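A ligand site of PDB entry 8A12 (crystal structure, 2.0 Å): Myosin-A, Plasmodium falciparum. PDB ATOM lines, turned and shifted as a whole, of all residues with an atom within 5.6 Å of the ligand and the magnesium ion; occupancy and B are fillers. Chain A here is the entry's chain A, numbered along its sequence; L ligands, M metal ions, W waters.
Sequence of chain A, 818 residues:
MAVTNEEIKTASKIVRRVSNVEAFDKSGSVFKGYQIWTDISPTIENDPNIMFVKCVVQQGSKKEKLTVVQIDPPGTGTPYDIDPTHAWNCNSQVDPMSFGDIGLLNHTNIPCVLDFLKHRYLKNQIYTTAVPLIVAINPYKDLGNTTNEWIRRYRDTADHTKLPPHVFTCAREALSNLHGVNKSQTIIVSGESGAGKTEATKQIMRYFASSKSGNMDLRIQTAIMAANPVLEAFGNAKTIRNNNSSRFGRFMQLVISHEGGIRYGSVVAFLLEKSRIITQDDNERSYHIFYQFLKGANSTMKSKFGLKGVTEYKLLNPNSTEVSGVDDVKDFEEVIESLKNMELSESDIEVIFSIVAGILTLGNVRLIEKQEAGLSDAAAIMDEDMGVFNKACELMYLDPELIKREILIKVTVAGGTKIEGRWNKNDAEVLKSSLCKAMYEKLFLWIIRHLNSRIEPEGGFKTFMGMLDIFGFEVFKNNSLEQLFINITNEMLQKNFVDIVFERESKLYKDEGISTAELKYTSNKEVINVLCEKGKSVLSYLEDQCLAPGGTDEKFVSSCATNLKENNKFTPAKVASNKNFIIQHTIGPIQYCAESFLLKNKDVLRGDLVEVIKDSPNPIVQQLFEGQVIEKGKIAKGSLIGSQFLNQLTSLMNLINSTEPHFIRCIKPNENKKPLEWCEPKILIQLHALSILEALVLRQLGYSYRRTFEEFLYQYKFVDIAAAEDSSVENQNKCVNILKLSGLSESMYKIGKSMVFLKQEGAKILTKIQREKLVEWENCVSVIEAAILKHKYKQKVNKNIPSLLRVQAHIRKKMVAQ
The magnesium ion is bound by water W4 (1.9 Å), the side-chain hydroxyl of Thr 198 (2.1 Å), an oxygen (O2) of the ligand (2.1 Å), water W6 (2.1 Å), the side-chain hydroxyl of Ser 246 (2.1 Å) and water W10 (2.1 Å).
The magnesium ion has six donor atoms within binding distance.
N of Tyr 140 lies within hydrogen-bond range of OD1 of Asn 138.
OG1 of Thr 198 sits close to OD2 of Asp 469 (2.8 Å).
The backbone NH (N) of Asn 244 sits at hydrogen-bond distance from the side-chain amide oxygen (OD1) of Asn 242 (2.8 Å).
OD1 of Asn 244 sits at hydrogen-bond distance from ND2 of Asn 236 (3.0 Å).
ND2 of Asn 138 is in hydrogen-bond range of O of Gly 194 (2.8 Å).
NZ of Lys 197 is in hydrogen-bond range of O of Glu 192 (3.1 Å).
The backbone carbonyl oxygen (O) of Gly 191 is in hydrogen-bond range of the side-chain amino group (NZ) of Lys 197, 3.0 Å away.
The side-chain hydroxyl of Tyr 140 is in hydrogen-bond range of the backbone carbonyl oxygen of Gly 194.
Water W4 lies within hydrogen-bond range of O4 of the ligand (2.8 Å), O of Asn 244 (2.9 Å) and N of Ser 246 (3.4 Å).
Water W10 lies within hydrogen-bond range of an oxygen (O1) of the ligand (2.5 Å) and the backbone NH of Ser 246 (2.8 Å).
Water W8 bridges N4 of the ligand (2.7 Å) and N of Leu 143 (3.2 Å).
Water W2 lies within hydrogen-bond range of OE2 of Glu 199, O4 of the ligand and ND2 of Asn 244.
Water W1 lies within hydrogen-bond range of O of Gly 196 (2.9 Å) and N3 of the ligand (3.3 Å).
Water W9 lies within hydrogen-bond range of O of Tyr 140 (3.3 Å) and O10 of the ligand (3.3 Å).
Of the 26 residues printed, 2 come within 4 Å of the magnesium ion.
Residues that only touch the ligand: Pro 139 (3.5 Å), Tyr 140 (3.5 Å), Lys 141 (3.1 Å), Glu 192 (3.7 Å), Ser 193 (3.8 Å) and Asn 244 (3.7 Å).
Hydrophobic or aromatic side chains that line the ligand: Pro 139 and Tyr 140.
Of the 26 residues printed, 15 come within 4 Å of the ligand.
The nearest printed residue that does not touch the ligand is Ser 246 (4.2 Å).
The side-chain amide nitrogen (ND2) of Asn 242 lies within hydrogen-bond range of an oxygen (O1) of the ligand (3.1 Å).
An oxygen (O3) of the ligand is in salt-bridge range of the side-chain amino group (NZ) of Lys 197 (2.7 Å).
The side-chain amide nitrogen (NE2) of Gln 203 sits close to a nitrogen (N3) of the ligand.
The backbone NH of Ala 195 sits at hydrogen-bond distance from an oxygen (O3) of the ligand (3.4 Å).
The backbone NH (N) of Gly 194 sits at hydrogen-bond distance from an oxygen (O1) of the ligand, 2.8 Å away.
An oxygen (O3) of the ligand sits at hydrogen-bond distance from the backbone NH of Lys 197 (2.8 Å).
An oxygen (O3) of the ligand sits at hydrogen-bond distance from the backbone NH (N) of Gly 196, 2.9 Å away.
An oxygen (O5) of the ligand lies within hydrogen-bond range of the backbone NH of Thr 198.
ND2 of Asn 138 sits at hydrogen-bond distance from O8 of the ligand.
O5 of the ligand sits at hydrogen-bond distance from N of Glu 199, 3.0 Å away.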
ATOM      1  N   ILE A 126       5.077   0.596 -17.292  1.00  0.00           N
ATOM      2  CA  ILE A 126       5.811   0.140 -18.469  1.00  0.00           C
ATOM      3  C   ILE A 126       5.349  -1.191 -19.012  1.00  0.00           C
ATOM      4  O   ILE A 126       5.867  -1.626 -20.026  1.00  0.00           O
ATOM      5  CB  ILE A 126       7.300   0.066 -18.192  1.00  0.00           C
ATOM      6  CG1 ILE A 126       7.610  -0.966 -17.096  1.00  0.00           C
ATOM      7  CG2 ILE A 126       7.830   1.445 -17.846  1.00  0.00           C
ATOM      8  CD1 ILE A 126       9.111  -1.146 -16.848  1.00  0.00           C
ATOM      9  N   TYR A 127       4.327  -1.810 -18.407  1.00  0.00           N
ATOM     10  CA  TYR A 127       3.855  -3.150 -18.700  1.00  0.00           C
ATOM     11  C   TYR A 127       2.403  -3.071 -19.125  1.00  0.00           C
ATOM     12  O   TYR A 127       1.616  -2.410 -18.458  1.00  0.00           O
ATOM     13  CB  TYR A 127       3.898  -4.044 -17.441  1.00  0.00           C
ATOM     14  CG  TYR A 127       5.245  -4.202 -16.812  1.00  0.00           C
ATOM     15  CD1 TYR A 127       6.278  -4.821 -17.484  1.00  0.00           C
ATOM     16  CD2 TYR A 127       5.486  -3.728 -15.503  1.00  0.00           C
ATOM     17  CE1 TYR A 127       7.539  -4.963 -16.905  1.00  0.00           C
ATOM     18  CE2 TYR A 127       6.777  -3.929 -14.877  1.00  0.00           C
ATOM     19  CZ  TYR A 127       7.784  -4.501 -15.627  1.00  0.00           C
ATOM     20  OH  TYR A 127       9.028  -4.650 -15.086  1.00  0.00           O
ATOM     21  N   ASN A 138      11.457  -0.592 -21.691  1.00  0.00           N
ATOM     22  CA  ASN A 138      12.601  -0.273 -20.850  1.00  0.00           C
ATOM     23  C   ASN A 138      12.527   1.162 -20.377  1.00  0.00           C
ATOM     24  O   ASN A 138      12.593   2.058 -21.206  1.00  0.00           O
ATOM     25  CB  ASN A 138      13.866  -0.513 -21.654  1.00  0.00           C
ATOM     26  CG  ASN A 138      15.111  -0.390 -20.835  1.00  0.00           C
ATOM     27  OD1 ASN A 138      15.064   0.121 -19.745  1.00  0.00           O
ATOM     28  ND2 ASN A 138      16.246  -0.852 -21.356  1.00  0.00           N
ATOM     29  N   PRO A 139      12.488   1.439 -19.060  1.00  0.00           N
ATOM     30  CA  PRO A 139      12.381   2.835 -18.589  1.00  0.00           C
ATOM     31  C   PRO A 139      13.719   3.508 -18.421  1.00  0.00           C
ATOM     32  O   PRO A 139      13.764   4.722 -18.155  1.00  0.00           O
ATOM     33  CB  PRO A 139      11.683   2.678 -17.231  1.00  0.00           C
ATOM     34  CG  PRO A 139      12.206   1.309 -16.744  1.00  0.00           C
ATOM     35  CD  PRO A 139      12.281   0.458 -17.987  1.00  0.00           C
ATOM     36  N   TYR A 140      14.797   2.751 -18.535  1.00  0.00           N
ATOM     37  CA  TYR A 140      16.178   3.255 -18.442  1.00  0.00           C
ATOM     38  C   TYR A 140      16.359   4.052 -17.165  1.00  0.00           C
ATOM     39  O   TYR A 140      17.118   5.022 -17.138  1.00  0.00           O
ATOM     40  CB  TYR A 140      16.608   4.055 -19.674  1.00  0.00           C
ATOM     41  CG  TYR A 140      17.117   3.179 -20.806  1.00  0.00           C
ATOM     42  CD1 TYR A 140      18.259   2.378 -20.651  1.00  0.00           C
ATOM     43  CD2 TYR A 140      16.456   3.127 -22.023  1.00  0.00           C
ATOM     44  CE1 TYR A 140      18.676   1.530 -21.694  1.00  0.00           C
ATOM     45  CE2 TYR A 140      16.884   2.299 -23.069  1.00  0.00           C
ATOM     46  CZ  TYR A 140      17.985   1.529 -22.917  1.00  0.00           C
ATOM     47  OH  TYR A 140      18.417   0.735 -23.984  1.00  0.00           O
ATOM     48  N   LYS A 141      15.644   3.662 -16.114  1.00  0.00           N
ATOM     49  CA  LYS A 141      15.858   4.166 -14.764  1.00  0.00           C
ATOM     50  C   LYS A 141      15.190   3.202 -13.812  1.00  0.00           C
ATOM     51  O   LYS A 141      14.267   2.483 -14.177  1.00  0.00           O
ATOM     52  CB  LYS A 141      15.312   5.570 -14.538  1.00  0.00           C
ATOM     53  CG  LYS A 141      13.815   5.740 -14.637  1.00  0.00           C
ATOM     54  CD  LYS A 141      13.429   7.151 -14.086  1.00  0.00           C
ATOM     55  CE  LYS A 141      12.390   7.917 -14.958  1.00  0.00           C
ATOM     56  NZ  LYS A 141      11.052   7.244 -15.126  1.00  0.00           N
ATOM     57  N   ASP A 142      15.682   3.185 -12.578  1.00  0.00           N
ATOM     58  CA  ASP A 142      15.030   2.353 -11.563  1.00  0.00           C
ATOM     59  C   ASP A 142      13.687   2.953 -11.166  1.00  0.00           C
ATOM     60  O   ASP A 142      13.624   3.965 -10.467  1.00  0.00           O
ATOM     61  CB  ASP A 142      15.936   2.223 -10.330  1.00  0.00           C
ATOM     62  CG  ASP A 142      15.472   1.086  -9.377  1.00  0.00           C
ATOM     63  OD1 ASP A 142      16.327   0.570  -8.642  1.00  0.00           O
ATOM     64  OD2 ASP A 142      14.272   0.661  -9.411  1.00  0.00           O
ATOM     65  N   LEU A 143      12.609   2.288 -11.554  1.00  0.00           N
ATOM     66  CA  LEU A 143      11.295   2.775 -11.200  1.00  0.00           C
ATOM     67  C   LEU A 143      10.886   2.411  -9.816  1.00  0.00           C
ATOM     68  O   LEU A 143       9.823   2.828  -9.380  1.00  0.00           O
ATOM     69  CB  LEU A 143      10.246   2.198 -12.169  1.00  0.00           C
ATOM     70  CG  LEU A 143      10.413   2.567 -13.662  1.00  0.00           C
ATOM     71  CD1 LEU A 143       9.280   1.994 -14.409  1.00  0.00           C
ATOM     72  CD2 LEU A 143      10.470   4.065 -13.720  1.00  0.00           C
ATOM     73  N   GLY A 191      13.145  -9.849 -27.470  1.00  0.00           N
ATOM     74  CA  GLY A 191      13.253  -8.435 -27.789  1.00  0.00           C
ATOM     75  C   GLY A 191      14.645  -8.136 -28.307  1.00  0.00           C
ATOM     76  O   GLY A 191      15.549  -8.971 -28.241  1.00  0.00           O
ATOM     77  N   GLU A 192      14.822  -6.917 -28.793  1.00  0.00           N
ATOM     78  CA  GLU A 192      16.099  -6.570 -29.370  1.00  0.00           C
ATOM     79  C   GLU A 192      17.053  -6.155 -28.250  1.00  0.00           C
ATOM     80  O   GLU A 192      16.676  -6.032 -27.084  1.00  0.00           O
ATOM     81  CB  GLU A 192      15.920  -5.487 -30.422  1.00  0.00           C
ATOM     82  CG  GLU A 192      15.504  -4.172 -29.914  1.00  0.00           C
ATOM     83  CD  GLU A 192      15.370  -3.128 -31.008  1.00  0.00           C
ATOM     84  OE1 GLU A 192      14.646  -3.330 -32.020  1.00  0.00           O
ATOM     85  OE2 GLU A 192      16.014  -2.076 -30.818  1.00  0.00           O
ATOM     86  N   SER A 193      18.319  -5.963 -28.650  1.00  0.00           N
ATOM     87  CA  SER A 193      19.387  -5.605 -27.732  1.00  0.00           C
ATOM     88  C   SER A 193      19.053  -4.368 -26.919  1.00  0.00           C
ATOM     89  O   SER A 193      18.708  -3.324 -27.465  1.00  0.00           O
ATOM     90  CB  SER A 193      20.683  -5.368 -28.519  1.00  0.00           C
ATOM     91  OG  SER A 193      21.816  -5.212 -27.618  1.00  0.00           O
ATOM     92  N   GLY A 194      19.264  -4.459 -25.602  1.00  0.00           N
ATOM     93  CA  GLY A 194      18.982  -3.321 -24.763  1.00  0.00           C
ATOM     94  C   GLY A 194      17.522  -3.114 -24.449  1.00  0.00           C
ATOM     95  O   GLY A 194      17.188  -2.174 -23.695  1.00  0.00           O
ATOM     96  N   ALA A 195      16.627  -4.032 -24.867  1.00  0.00           N
ATOM     97  CA  ALA A 195      15.207  -3.858 -24.536  1.00  0.00           C
ATOM     98  C   ALA A 195      14.811  -4.245 -23.119  1.00  0.00           C
ATOM     99  O   ALA A 195      13.743  -3.862 -22.662  1.00  0.00           O
ATOM    100  CB  ALA A 195      14.352  -4.626 -25.514  1.00  0.00           C
ATOM    101  N   GLY A 196      15.633  -5.037 -22.419  1.00  0.00           N
ATOM    102  CA  GLY A 196      15.357  -5.320 -21.021  1.00  0.00           C
ATOM    103  C   GLY A 196      15.074  -6.769 -20.679  1.00  0.00           C
ATOM    104  O   GLY A 196      14.524  -7.035 -19.626  1.00  0.00           O
ATOM    105  N   LYS A 197      15.451  -7.697 -21.552  1.00  0.00           N
ATOM    106  CA  LYS A 197      15.110  -9.090 -21.331  1.00  0.00           C
ATOM    107  C   LYS A 197      15.829  -9.669 -20.122  1.00  0.00           C
ATOM    108  O   LYS A 197      15.251 -10.475 -19.366  1.00  0.00           O
ATOM    109  CB  LYS A 197      15.526  -9.919 -22.529  1.00  0.00           C
ATOM    110  CG  LYS A 197      15.187  -9.329 -23.880  1.00  0.00           C
ATOM    111  CD  LYS A 197      15.570 -10.387 -24.995  1.00  0.00           C
ATOM    112  CE  LYS A 197      17.033 -10.240 -25.296  1.00  0.00           C
ATOM    113  NZ  LYS A 197      17.240  -8.793 -25.742  1.00  0.00           N
ATOM    114  N   THR A 198      17.100  -9.345 -19.947  1.00  0.00           N
ATOM    115  CA  THR A 198      17.868  -9.964 -18.868  1.00  0.00           C
ATOM    116  C   THR A 198      17.453  -9.369 -17.536  1.00  0.00           C
ATOM    117  O   THR A 198      17.390 -10.084 -16.535  1.00  0.00           O
ATOM    118  CB  THR A 198      19.343  -9.751 -19.162  1.00  0.00           C
ATOM    119  OG1 THR A 198      19.671 -10.469 -20.356  1.00  0.00           O
ATOM    120  CG2 THR A 198      20.230 -10.256 -18.034  1.00  0.00           C
ATOM    121  N   GLU A 199      17.140  -8.075 -17.512  1.00  0.00           N
ATOM    122  CA  GLU A 199      16.613  -7.488 -16.280  1.00  0.00           C
ATOM    123  C   GLU A 199      15.275  -8.099 -15.916  1.00  0.00           C
ATOM    124  O   GLU A 199      15.018  -8.446 -14.754  1.00  0.00           O
ATOM    125  CB  GLU A 199      16.474  -5.962 -16.441  1.00  0.00           C
ATOM    126  CG  GLU A 199      17.812  -5.215 -16.496  1.00  0.00           C
ATOM    127  CD  GLU A 199      18.820  -5.657 -15.387  1.00  0.00           C
ATOM    128  OE1 GLU A 199      18.442  -5.521 -14.168  1.00  0.00           O
ATOM    129  OE2 GLU A 199      19.984  -6.061 -15.759  1.00  0.00           O
ATOM    130  N   ALA A 200      14.399  -8.251 -16.901  1.00  0.00           N
ATOM    131  CA  ALA A 200      13.114  -8.883 -16.605  1.00  0.00           C
ATOM    132  C   ALA A 200      13.298 -10.286 -16.035  1.00  0.00           C
ATOM    133  O   ALA A 200      12.627 -10.687 -15.079  1.00  0.00           O
ATOM    134  CB  ALA A 200      12.292  -8.933 -17.885  1.00  0.00           C
ATOM    135  N   GLN A 203      14.344 -10.159 -12.523  1.00  0.00           N
ATOM    136  CA  GLN A 203      13.248  -9.753 -11.658  1.00  0.00           C
ATOM    137  C   GLN A 203      12.326 -10.930 -11.350  1.00  0.00           C
ATOM    138  O   GLN A 203      11.880 -11.112 -10.226  1.00  0.00           O
ATOM    139  CB  GLN A 203      12.448  -8.617 -12.310  1.00  0.00           C
ATOM    140  CG  GLN A 203      13.256  -7.323 -12.354  1.00  0.00           C
ATOM    141  CD  GLN A 203      12.829  -6.406 -13.499  1.00  0.00           C
ATOM    142  OE1 GLN A 203      11.801  -6.633 -14.144  1.00  0.00           O
ATOM    143  NE2 GLN A 203      13.614  -5.352 -13.736  1.00  0.00           N
ATOM    144  N   ASN A 236      28.559 -11.589 -21.159  1.00  0.00           N
ATOM    145  CA  ASN A 236      28.003 -10.301 -21.527  1.00  0.00           C
ATOM    146  C   ASN A 236      29.145  -9.337 -21.805  1.00  0.00           C
ATOM    147  O   ASN A 236      30.226  -9.453 -21.249  1.00  0.00           O
ATOM    148  CB  ASN A 236      27.151  -9.695 -20.418  1.00  0.00           C
ATOM    149  CG  ASN A 236      25.779 -10.392 -20.246  1.00  0.00           C
ATOM    150  OD1 ASN A 236      25.611 -11.571 -20.596  1.00  0.00           O
ATOM    151  ND2 ASN A 236      24.821  -9.653 -19.706  1.00  0.00           N
ATOM    152  N   ASN A 242      24.096  -1.776 -25.859  1.00  0.00           N
ATOM    153  CA  ASN A 242      23.839  -2.194 -24.487  1.00  0.00           C
ATOM    154  C   ASN A 242      25.156  -2.336 -23.747  1.00  0.00           C
ATOM    155  O   ASN A 242      26.013  -3.140 -24.116  1.00  0.00           O
ATOM    156  CB  ASN A 242      23.043  -3.497 -24.502  1.00  0.00           C
ATOM    157  CG  ASN A 242      22.588  -3.953 -23.109  1.00  0.00           C
ATOM    158  OD1 ASN A 242      22.888  -3.333 -22.050  1.00  0.00           O
ATOM    159  ND2 ASN A 242      21.859  -5.044 -23.101  1.00  0.00           N
ATOM    160  N   ASN A 244      25.559  -3.809 -21.235  1.00  0.00           N
ATOM    161  CA  ASN A 244      25.536  -5.162 -20.620  1.00  0.00           C
ATOM    162  C   ASN A 244      24.853  -6.173 -21.532  1.00  0.00           C
ATOM    163  O   ASN A 244      23.943  -6.878 -21.136  1.00  0.00           O
ATOM    164  CB  ASN A 244      24.824  -5.146 -19.271  1.00  0.00           C
ATOM    165  CG  ASN A 244      25.008  -6.424 -18.496  1.00  0.00           C
ATOM    166  OD1 ASN A 244      26.005  -7.121 -18.615  1.00  0.00           O
ATOM    167  ND2 ASN A 244      24.040  -6.729 -17.668  1.00  0.00           N
ATOM    168  N   SER A 245      25.298  -6.238 -22.793  1.00  0.00           N
ATOM    169  CA  SER A 245      24.668  -7.065 -23.818  1.00  0.00           C
ATOM    170  C   SER A 245      24.960  -8.526 -23.545  1.00  0.00           C
ATOM    171  O   SER A 245      26.121  -8.894 -23.404  1.00  0.00           O
ATOM    172  CB  SER A 245      25.197  -6.666 -25.205  1.00  0.00           C
ATOM    173  OG  SER A 245      24.803  -7.509 -26.283  1.00  0.00           O
ATOM    174  N   SER A 246      23.905  -9.343 -23.443  1.00  0.00           N
ATOM    175  CA  SER A 246      24.078 -10.788 -23.402  1.00  0.00           C
ATOM    176  C   SER A 246      24.529 -11.309 -24.753  1.00  0.00           C
ATOM    177  O   SER A 246      23.862 -11.094 -25.758  1.00  0.00           O
ATOM    178  CB  SER A 246      22.790 -11.502 -23.021  1.00  0.00           C
ATOM    179  OG  SER A 246      22.121 -10.796 -21.950  1.00  0.00           O
ATOM    180  N   ASP A 469      15.686 -16.538 -22.306  1.00  0.00           N
ATOM    181  CA  ASP A 469      16.115 -15.141 -22.429  1.00  0.00           C
ATOM    182  C   ASP A 469      16.947 -15.109 -23.692  1.00  0.00           C
ATOM    183  O   ASP A 469      18.119 -15.508 -23.658  1.00  0.00           O
ATOM    184  CB  ASP A 469      16.954 -14.720 -21.211  1.00  0.00           C
ATOM    185  CG  ASP A 469      17.563 -13.343 -21.339  1.00  0.00           C
ATOM    186  OD1 ASP A 469      17.190 -12.650 -22.302  1.00  0.00           O
ATOM    187  OD2 ASP A 469      18.418 -12.935 -20.469  1.00  0.00           O
ATOM    188  N   CYS A 666       9.862  -7.432 -24.923  1.00  0.00           N
ATOM    189  CA  CYS A 666      10.458  -6.213 -24.376  1.00  0.00           C
ATOM    190  C   CYS A 666      10.706  -5.213 -25.487  1.00  0.00           C
ATOM    191  O   CYS A 666      11.145  -5.597 -26.573  1.00  0.00           O
ATOM    192  CB  CYS A 666      11.782  -6.515 -23.668  1.00  0.00           C
ATOM    193  SG  CYS A 666      11.571  -7.573 -22.235  1.00  0.00           S
HETATM  194  P1  LIG L   1      18.644  -7.049 -23.069  1.00  0.00           P
HETATM  195  O1  LIG L   1      19.662  -6.875 -24.167  1.00  0.00           O
HETATM  196  O2  LIG L   1      18.909  -8.168 -22.137  1.00  0.00           O
HETATM  197  O3  LIG L   1      17.284  -7.078 -23.635  1.00  0.00           O
HETATM  198  P2  LIG L   1      18.935  -5.640 -20.647  1.00  0.00           P
HETATM  199  O4  LIG L   1      20.376  -6.043 -20.432  1.00  0.00           O
HETATM  200  O5  LIG L   1      18.009  -6.369 -19.809  1.00  0.00           O
HETATM  201  O6  LIG L   1      18.556  -5.733 -22.209  1.00  0.00           O
HETATM  202  O7  LIG L   1      18.707  -4.037 -20.385  1.00  0.00           O
HETATM  203  C1  LIG L   1      19.769  -3.238 -20.757  1.00  0.00           C
HETATM  204  C2  LIG L   1      19.727  -2.044 -19.783  1.00  0.00           C
HETATM  205  O8  LIG L   1      18.551  -1.393 -19.802  1.00  0.00           O
HETATM  206  C3  LIG L   1      19.934  -2.556 -18.319  1.00  0.00           C
HETATM  207  O9  LIG L   1      21.264  -2.751 -18.001  1.00  0.00           O
HETATM  208  C4  LIG L   1      19.219  -1.439 -17.565  1.00  0.00           C
HETATM  209  O10 LIG L   1      20.168  -0.277 -17.537  1.00  0.00           O
HETATM  210  C5  LIG L   1      18.222  -1.006 -18.286  1.00  0.00           C
HETATM  211  N1  LIG L   1      16.995  -1.718 -18.025  1.00  0.00           N
HETATM  212  C6  LIG L   1      16.476  -2.799 -18.643  1.00  0.00           C
HETATM  213  N2  LIG L   1      15.310  -3.148 -18.068  1.00  0.00           N
HETATM  214  C7  LIG L   1      15.134  -2.265 -17.061  1.00  0.00           C
HETATM  215  C8  LIG L   1      14.142  -2.165 -16.166  1.00  0.00           C
HETATM  216  N3  LIG L   1      12.978  -2.975 -16.053  1.00  0.00           N
HETATM  217  N4  LIG L   1      14.087  -1.235 -15.217  1.00  0.00           N
HETATM  218  C9  LIG L   1      15.120  -0.350 -15.169  1.00  0.00           C
HETATM  219  N5  LIG L   1      16.181  -0.430 -16.028  1.00  0.00           N
HETATM  220  C10 LIG L   1      16.152  -1.387 -17.014  1.00  0.00           C
HETATM  221 MG    MG M   1      20.333  -9.670 -22.142  1.00  0.00          MG
HETATM  222  O   HOH W   1      12.628  -5.131 -18.496  1.00  0.00           O
HETATM  223  O   HOH W   2      21.481  -5.581 -17.918  1.00  0.00           O
HETATM  224  O   HOH W   3      23.512  -1.577 -19.006  1.00  0.00           O
HETATM  225  O   HOH W   4      21.483  -8.425 -21.267  1.00  0.00           O
HETATM  226  O   HOH W   5      18.193   1.210 -14.906  1.00  0.00           O
HETATM  227  O   HOH W   6      19.363 -11.291 -22.999  1.00  0.00           O
HETATM  228  O   HOH W   7      21.947  -0.393 -15.166  1.00  0.00           O
HETATM  229  O   HOH W   8      12.510  -0.456 -13.147  1.00  0.00           O
HETATM  230  O   HOH W   9      19.563   2.867 -16.740  1.00  0.00           O
HETATM  231  O   HOH W  10      21.178  -8.906 -23.950  1.00  0.00           O
